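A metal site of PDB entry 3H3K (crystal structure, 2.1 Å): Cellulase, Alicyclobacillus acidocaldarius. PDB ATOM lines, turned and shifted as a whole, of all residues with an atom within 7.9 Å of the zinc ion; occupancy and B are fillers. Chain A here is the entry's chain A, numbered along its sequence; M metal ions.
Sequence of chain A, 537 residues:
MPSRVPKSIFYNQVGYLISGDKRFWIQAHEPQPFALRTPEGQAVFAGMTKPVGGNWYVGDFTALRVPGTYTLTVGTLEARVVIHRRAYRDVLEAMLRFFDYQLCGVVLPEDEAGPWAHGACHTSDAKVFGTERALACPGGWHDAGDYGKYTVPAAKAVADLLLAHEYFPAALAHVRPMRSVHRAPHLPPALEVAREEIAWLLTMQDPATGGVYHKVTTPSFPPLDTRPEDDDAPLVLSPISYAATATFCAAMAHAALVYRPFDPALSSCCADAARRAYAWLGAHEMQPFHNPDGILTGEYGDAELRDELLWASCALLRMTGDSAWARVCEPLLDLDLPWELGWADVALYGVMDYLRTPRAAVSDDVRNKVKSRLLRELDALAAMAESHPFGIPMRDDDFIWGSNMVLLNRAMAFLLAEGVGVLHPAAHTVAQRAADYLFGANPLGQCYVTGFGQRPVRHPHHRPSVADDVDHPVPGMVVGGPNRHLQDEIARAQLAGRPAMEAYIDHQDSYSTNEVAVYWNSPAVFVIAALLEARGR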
ATOM      1  N   GLN A 102     -20.791   9.823 -18.320  1.00  0.00           N
ATOM      2  CA  GLN A 102     -19.705   8.859 -18.544  1.00  0.00           C
ATOM      3  C   GLN A 102     -19.026   8.412 -17.259  1.00  0.00           C
ATOM      4  O   GLN A 102     -18.122   7.575 -17.300  1.00  0.00           O
ATOM      5  CB  GLN A 102     -18.643   9.444 -19.491  1.00  0.00           C
ATOM      6  CG  GLN A 102     -19.096   9.684 -20.920  1.00  0.00           C
ATOM      7  CD  GLN A 102     -19.312   8.405 -21.707  1.00  0.00           C
ATOM      8  OE1 GLN A 102     -20.381   7.827 -21.681  1.00  0.00           O
ATOM      9  NE2 GLN A 102     -18.283   7.955 -22.423  1.00  0.00           N
ATOM     10  N   LEU A 103     -19.425   8.956 -16.109  1.00  0.00           N
ATOM     11  CA  LEU A 103     -18.742   8.620 -14.853  1.00  0.00           C
ATOM     12  C   LEU A 103     -18.721   7.106 -14.603  1.00  0.00           C
ATOM     13  O   LEU A 103     -19.728   6.410 -14.808  1.00  0.00           O
ATOM     14  CB  LEU A 103     -19.357   9.346 -13.653  1.00  0.00           C
ATOM     15  CG  LEU A 103     -18.927  10.789 -13.437  1.00  0.00           C
ATOM     16  CD1 LEU A 103     -19.815  11.425 -12.378  1.00  0.00           C
ATOM     17  CD2 LEU A 103     -17.447  10.876 -13.053  1.00  0.00           C
ATOM     18  N   CYS A 104     -17.568   6.631 -14.150  1.00  0.00           N
ATOM     19  CA  CYS A 104     -17.360   5.237 -13.814  1.00  0.00           C
ATOM     20  C   CYS A 104     -17.207   5.096 -12.298  1.00  0.00           C
ATOM     21  O   CYS A 104     -16.539   5.902 -11.658  1.00  0.00           O
ATOM     22  CB  CYS A 104     -16.097   4.742 -14.509  1.00  0.00           C
ATOM     23  SG  CYS A 104     -15.795   2.996 -14.289  1.00  0.00           S
ATOM     24  N   GLY A 105     -17.838   4.061 -11.731  1.00  0.00           N
ATOM     25  CA  GLY A 105     -17.680   3.734 -10.309  1.00  0.00           C
ATOM     26  C   GLY A 105     -18.467   4.618  -9.358  1.00  0.00           C
ATOM     27  O   GLY A 105     -18.126   4.708  -8.176  1.00  0.00           O
ATOM     28  N   VAL A 106     -19.518   5.258  -9.865  1.00  0.00           N
ATOM     29  CA  VAL A 106     -20.367   6.139  -9.063  1.00  0.00           C
ATOM     30  C   VAL A 106     -21.837   5.941  -9.431  1.00  0.00           C
ATOM     31  O   VAL A 106     -22.175   5.740 -10.605  1.00  0.00           O
ATOM     32  CB  VAL A 106     -19.998   7.630  -9.248  1.00  0.00           C
ATOM     33  CG1 VAL A 106     -18.490   7.843  -9.169  1.00  0.00           C
ATOM     34  CG2 VAL A 106     -20.529   8.153 -10.578  1.00  0.00           C
ATOM     35  N   HIS A 118     -27.805   4.608 -13.204  1.00  0.00           N
ATOM     36  CA  HIS A 118     -27.280   3.274 -12.898  1.00  0.00           C
ATOM     37  C   HIS A 118     -26.449   3.261 -11.625  1.00  0.00           C
ATOM     38  O   HIS A 118     -26.012   4.309 -11.130  1.00  0.00           O
ATOM     39  CB  HIS A 118     -26.484   2.692 -14.089  1.00  0.00           C
ATOM     40  CG  HIS A 118     -25.197   3.409 -14.383  1.00  0.00           C
ATOM     41  ND1 HIS A 118     -24.038   3.182 -13.664  1.00  0.00           N
ATOM     42  CD2 HIS A 118     -24.893   4.335 -15.319  1.00  0.00           C
ATOM     43  CE1 HIS A 118     -23.077   3.950 -14.142  1.00  0.00           C
ATOM     44  NE2 HIS A 118     -23.559   4.660 -15.151  1.00  0.00           N
ATOM     45  N   GLY A 119     -26.227   2.058 -11.088  1.00  0.00           N
ATOM     46  CA  GLY A 119     -25.391   1.880  -9.908  1.00  0.00           C
ATOM     47  C   GLY A 119     -23.924   1.906 -10.299  1.00  0.00           C
ATOM     48  O   GLY A 119     -23.599   1.793 -11.492  1.00  0.00           O
ATOM     49  N   ALA A 120     -23.045   2.049  -9.309  1.00  0.00           N
ATOM     50  CA  ALA A 120     -21.609   2.136  -9.541  1.00  0.00           C
ATOM     51  C   ALA A 120     -21.092   0.926 -10.334  1.00  0.00           C
ATOM     52  O   ALA A 120     -21.357  -0.210  -9.975  1.00  0.00           O
ATOM     53  CB  ALA A 120     -20.860   2.269  -8.226  1.00  0.00           C
ATOM     54  N   CYS A 121     -20.367   1.198 -11.419  1.00  0.00           N
ATOM     55  CA  CYS A 121     -19.825   0.164 -12.302  1.00  0.00           C
ATOM     56  C   CYS A 121     -18.310   0.044 -12.155  1.00  0.00           C
ATOM     57  O   CYS A 121     -17.657   0.956 -11.651  1.00  0.00           O
ATOM     58  CB  CYS A 121     -20.173   0.478 -13.762  1.00  0.00           C
ATOM     59  SG  CYS A 121     -19.835   2.184 -14.262  1.00  0.00           S
ATOM     60  N   HIS A 122     -17.776  -1.093 -12.597  1.00  0.00           N
ATOM     61  CA  HIS A 122     -16.333  -1.367 -12.606  1.00  0.00           C
ATOM     62  C   HIS A 122     -15.659  -1.087 -11.256  1.00  0.00           C
ATOM     63  O   HIS A 122     -14.592  -0.473 -11.196  1.00  0.00           O
ATOM     64  CB  HIS A 122     -15.656  -0.574 -13.730  1.00  0.00           C
ATOM     65  CG  HIS A 122     -16.268  -0.813 -15.070  1.00  0.00           C
ATOM     66  ND1 HIS A 122     -17.134   0.086 -15.655  1.00  0.00           N
ATOM     67  CD2 HIS A 122     -16.179  -1.860 -15.915  1.00  0.00           C
ATOM     68  CE1 HIS A 122     -17.536  -0.397 -16.815  1.00  0.00           C
ATOM     69  NE2 HIS A 122     -16.982  -1.576 -16.997  1.00  0.00           N
ATOM     70  N   THR A 123     -16.279  -1.576 -10.195  1.00  0.00           N
ATOM     71  CA  THR A 123     -15.838  -1.302  -8.826  1.00  0.00           C
ATOM     72  C   THR A 123     -14.654  -2.168  -8.357  1.00  0.00           C
ATOM     73  O   THR A 123     -14.019  -1.862  -7.346  1.00  0.00           O
ATOM     74  CB  THR A 123     -17.017  -1.441  -7.836  1.00  0.00           C
ATOM     75  OG1 THR A 123     -17.735  -2.646  -8.114  1.00  0.00           O
ATOM     76  CG2 THR A 123     -17.964  -0.255  -7.983  1.00  0.00           C
ATOM     77  N   GLY A 139     -13.310   5.603 -10.480  1.00  0.00           N
ATOM     78  CA  GLY A 139     -13.672   6.954 -10.847  1.00  0.00           C
ATOM     79  C   GLY A 139     -13.341   7.264 -12.288  1.00  0.00           C
ATOM     80  O   GLY A 139     -13.051   6.369 -13.074  1.00  0.00           O
ATOM     81  N   GLY A 140     -13.376   8.542 -12.628  1.00  0.00           N
ATOM     82  CA  GLY A 140     -13.071   8.998 -13.984  1.00  0.00           C
ATOM     83  C   GLY A 140     -14.188   8.728 -14.969  1.00  0.00           C
ATOM     84  O   GLY A 140     -15.324   8.461 -14.587  1.00  0.00           O
ATOM     85  N   TRP A 141     -13.838   8.791 -16.251  1.00  0.00           N
ATOM     86  CA  TRP A 141     -14.832   8.719 -17.324  1.00  0.00           C
ATOM     87  C   TRP A 141     -14.604   7.506 -18.183  1.00  0.00           C
ATOM     88  O   TRP A 141     -13.461   7.158 -18.489  1.00  0.00           O
ATOM     89  CB  TRP A 141     -14.740   9.959 -18.239  1.00  0.00           C
ATOM     90  CG  TRP A 141     -15.004  11.250 -17.554  1.00  0.00           C
ATOM     91  CD1 TRP A 141     -15.974  11.500 -16.621  1.00  0.00           C
ATOM     92  CD2 TRP A 141     -14.297  12.479 -17.742  1.00  0.00           C
ATOM     93  NE1 TRP A 141     -15.910  12.804 -16.216  1.00  0.00           N
ATOM     94  CE2 TRP A 141     -14.886  13.433 -16.885  1.00  0.00           C
ATOM     95  CE3 TRP A 141     -13.224  12.877 -18.564  1.00  0.00           C
ATOM     96  CZ2 TRP A 141     -14.452  14.763 -16.815  1.00  0.00           C
ATOM     97  CZ3 TRP A 141     -12.783  14.196 -18.487  1.00  0.00           C
ATOM     98  CH2 TRP A 141     -13.393  15.119 -17.611  1.00  0.00           C
ATOM     99  N   HIS A 142     -15.695   6.867 -18.570  1.00  0.00           N
ATOM    100  CA  HIS A 142     -15.656   5.962 -19.698  1.00  0.00           C
ATOM    101  C   HIS A 142     -15.285   6.832 -20.898  1.00  0.00           C
ATOM    102  O   HIS A 142     -15.895   7.871 -21.156  1.00  0.00           O
ATOM    103  CB  HIS A 142     -17.010   5.300 -19.940  1.00  0.00           C
ATOM    104  CG  HIS A 142     -17.525   4.528 -18.765  1.00  0.00           C
ATOM    105  ND1 HIS A 142     -18.845   4.576 -18.376  1.00  0.00           N
ATOM    106  CD2 HIS A 142     -16.897   3.698 -17.888  1.00  0.00           C
ATOM    107  CE1 HIS A 142     -19.013   3.798 -17.318  1.00  0.00           C
ATOM    108  NE2 HIS A 142     -17.843   3.260 -16.996  1.00  0.00           N
ATOM    109  N   ASP A 146     -17.182   2.713 -25.423  1.00  0.00           N
ATOM    110  CA  ASP A 146     -16.759   1.600 -24.576  1.00  0.00           C
ATOM    111  C   ASP A 146     -16.598   2.032 -23.109  1.00  0.00           C
ATOM    112  O   ASP A 146     -16.926   3.168 -22.757  1.00  0.00           O
ATOM    113  CB  ASP A 146     -15.452   1.008 -25.119  1.00  0.00           C
ATOM    114  CG  ASP A 146     -14.245   1.885 -24.826  1.00  0.00           C
ATOM    115  OD1 ASP A 146     -14.337   3.105 -25.042  1.00  0.00           O
ATOM    116  OD2 ASP A 146     -13.196   1.337 -24.356  1.00  0.00           O
ATOM    117  N   TYR A 147     -16.103   1.141 -22.257  1.00  0.00           N
ATOM    118  CA  TYR A 147     -15.968   1.443 -20.825  1.00  0.00           C
ATOM    119  C   TYR A 147     -14.540   1.585 -20.333  1.00  0.00           C
ATOM    120  O   TYR A 147     -14.314   1.782 -19.146  1.00  0.00           O
ATOM    121  CB  TYR A 147     -16.728   0.412 -19.990  1.00  0.00           C
ATOM    122  CG  TYR A 147     -18.210   0.390 -20.300  1.00  0.00           C
ATOM    123  CD1 TYR A 147     -18.960   1.552 -20.276  1.00  0.00           C
ATOM    124  CD2 TYR A 147     -18.857  -0.800 -20.647  1.00  0.00           C
ATOM    125  CE1 TYR A 147     -20.323   1.564 -20.576  1.00  0.00           C
ATOM    126  CE2 TYR A 147     -20.227  -0.809 -20.956  1.00  0.00           C
ATOM    127  CZ  TYR A 147     -20.949   0.373 -20.917  1.00  0.00           C
ATOM    128  OH  TYR A 147     -22.297   0.375 -21.217  1.00  0.00           O
ATOM    129  N   GLY A 148     -13.575   1.513 -21.242  1.00  0.00           N
ATOM    130  CA  GLY A 148     -12.168   1.701 -20.896  1.00  0.00           C
ATOM    131  C   GLY A 148     -11.867   3.131 -20.497  1.00  0.00           C
ATOM    132  O   GLY A 148     -12.565   4.064 -20.881  1.00  0.00           O
ATOM    133  N   LYS A 149     -10.831   3.297 -19.688  1.00  0.00           N
ATOM    134  CA  LYS A 149     -10.357   4.610 -19.279  1.00  0.00           C
ATOM    135  C   LYS A 149      -8.892   4.697 -19.681  1.00  0.00           C
ATOM    136  O   LYS A 149      -8.076   3.884 -19.255  1.00  0.00           O
ATOM    137  CB  LYS A 149     -10.552   4.791 -17.764  1.00  0.00           C
ATOM    138  CG  LYS A 149     -11.962   4.433 -17.311  1.00  0.00           C
ATOM    139  CD  LYS A 149     -12.261   4.855 -15.883  1.00  0.00           C
ATOM    140  CE  LYS A 149     -11.742   3.827 -14.875  1.00  0.00           C
ATOM    141  NZ  LYS A 149     -12.339   4.025 -13.511  1.00  0.00           N
ATOM    142  N   PRO A 228     -23.297  -0.586 -18.306  1.00  0.00           N
ATOM    143  CA  PRO A 228     -22.013  -0.398 -17.614  1.00  0.00           C
ATOM    144  C   PRO A 228     -21.855  -1.267 -16.361  1.00  0.00           C
ATOM    145  O   PRO A 228     -20.788  -1.862 -16.149  1.00  0.00           O
ATOM    146  CB  PRO A 228     -22.003   1.097 -17.249  1.00  0.00           C
ATOM    147  CG  PRO A 228     -23.414   1.560 -17.407  1.00  0.00           C
ATOM    148  CD  PRO A 228     -24.062   0.662 -18.405  1.00  0.00           C
ATOM    149  N   GLU A 229     -22.907  -1.334 -15.551  1.00  0.00           N
ATOM    150  CA  GLU A 229     -22.865  -2.096 -14.293  1.00  0.00           C
ATOM    151  C   GLU A 229     -22.903  -3.629 -14.504  1.00  0.00           C
ATOM    152  O   GLU A 229     -22.497  -4.384 -13.618  1.00  0.00           O
ATOM    153  CB  GLU A 229     -23.973  -1.651 -13.316  1.00  0.00           C
ATOM    154  CG  GLU A 229     -25.398  -1.976 -13.747  1.00  0.00           C
ATOM    155  CD  GLU A 229     -26.007  -0.981 -14.721  1.00  0.00           C
ATOM    156  OE1 GLU A 229     -25.290  -0.468 -15.611  1.00  0.00           O
ATOM    157  OE2 GLU A 229     -27.217  -0.706 -14.604  1.00  0.00           O
ATOM    158  N   ASP A 231     -21.093  -5.067 -16.912  1.00  0.00           N
ATOM    159  CA  ASP A 231     -19.764  -5.419 -17.429  1.00  0.00           C
ATOM    160  C   ASP A 231     -18.830  -5.863 -16.297  1.00  0.00           C
ATOM    161  O   ASP A 231     -18.290  -5.034 -15.572  1.00  0.00           O
ATOM    162  CB  ASP A 231     -19.171  -4.215 -18.193  1.00  0.00           C
ATOM    163  CG  ASP A 231     -17.767  -4.474 -18.726  1.00  0.00           C
ATOM    164  OD1 ASP A 231     -17.383  -5.647 -18.909  1.00  0.00           O
ATOM    165  OD2 ASP A 231     -17.053  -3.473 -18.968  1.00  0.00           O
ATOM    166  N   LEU A 235     -10.653  -6.106 -14.781  1.00  0.00           N
ATOM    167  CA  LEU A 235      -9.985  -4.905 -15.255  1.00  0.00           C
ATOM    168  C   LEU A 235      -8.480  -5.127 -15.268  1.00  0.00           C
ATOM    169  O   LEU A 235      -7.937  -5.701 -14.330  1.00  0.00           O
ATOM    170  CB  LEU A 235     -10.319  -3.716 -14.348  1.00  0.00           C
ATOM    171  CG  LEU A 235     -11.786  -3.281 -14.366  1.00  0.00           C
ATOM    172  CD1 LEU A 235     -12.027  -2.217 -13.317  1.00  0.00           C
ATOM    173  CD2 LEU A 235     -12.196  -2.801 -15.761  1.00  0.00           C
HETATM  174 ZN    ZN M   1     -17.575   2.119 -15.267  1.00  0.00          ZN
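The side-chain amide nitrogen (NE2) of Gln 102 lies within hydrogen-bond range of the backbone carbonyl oxygen (O) of His 142.
A ring nitrogen (NE2) of His 122 is in hydrogen-bond range of the side-chain carboxylate (OD2) of Asp 231, 2.7 Å away.
SG of Cys 104 lies close to NZ of Lys 149 (3.7 Å).
O of Cys 104 sits close to N of Gly 139, at 3.5 Å.
N of Cys 104 is in hydrogen-bond range of O of Gly 140 (2.9 Å).
The backbone carbonyl oxygen (O) of Cys 121 sits close to the backbone NH (N) of Gly 105 (3.1 Å).
Within 4 Å of the zinc ion: Cys 104, Cys 121, His 122 and His 142.
NE2 of His 142 is bound to the zinc ion, 2.1 Å away.
ND1 of His 122 binds the zinc ion (2.1 Å).
The zinc ion is bound by SG of Cys 104 (2.2 Å).
The zinc ion is bound by SG of Cys 121 (2.5 Å).
The zinc ion has four donor atoms within binding distance.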
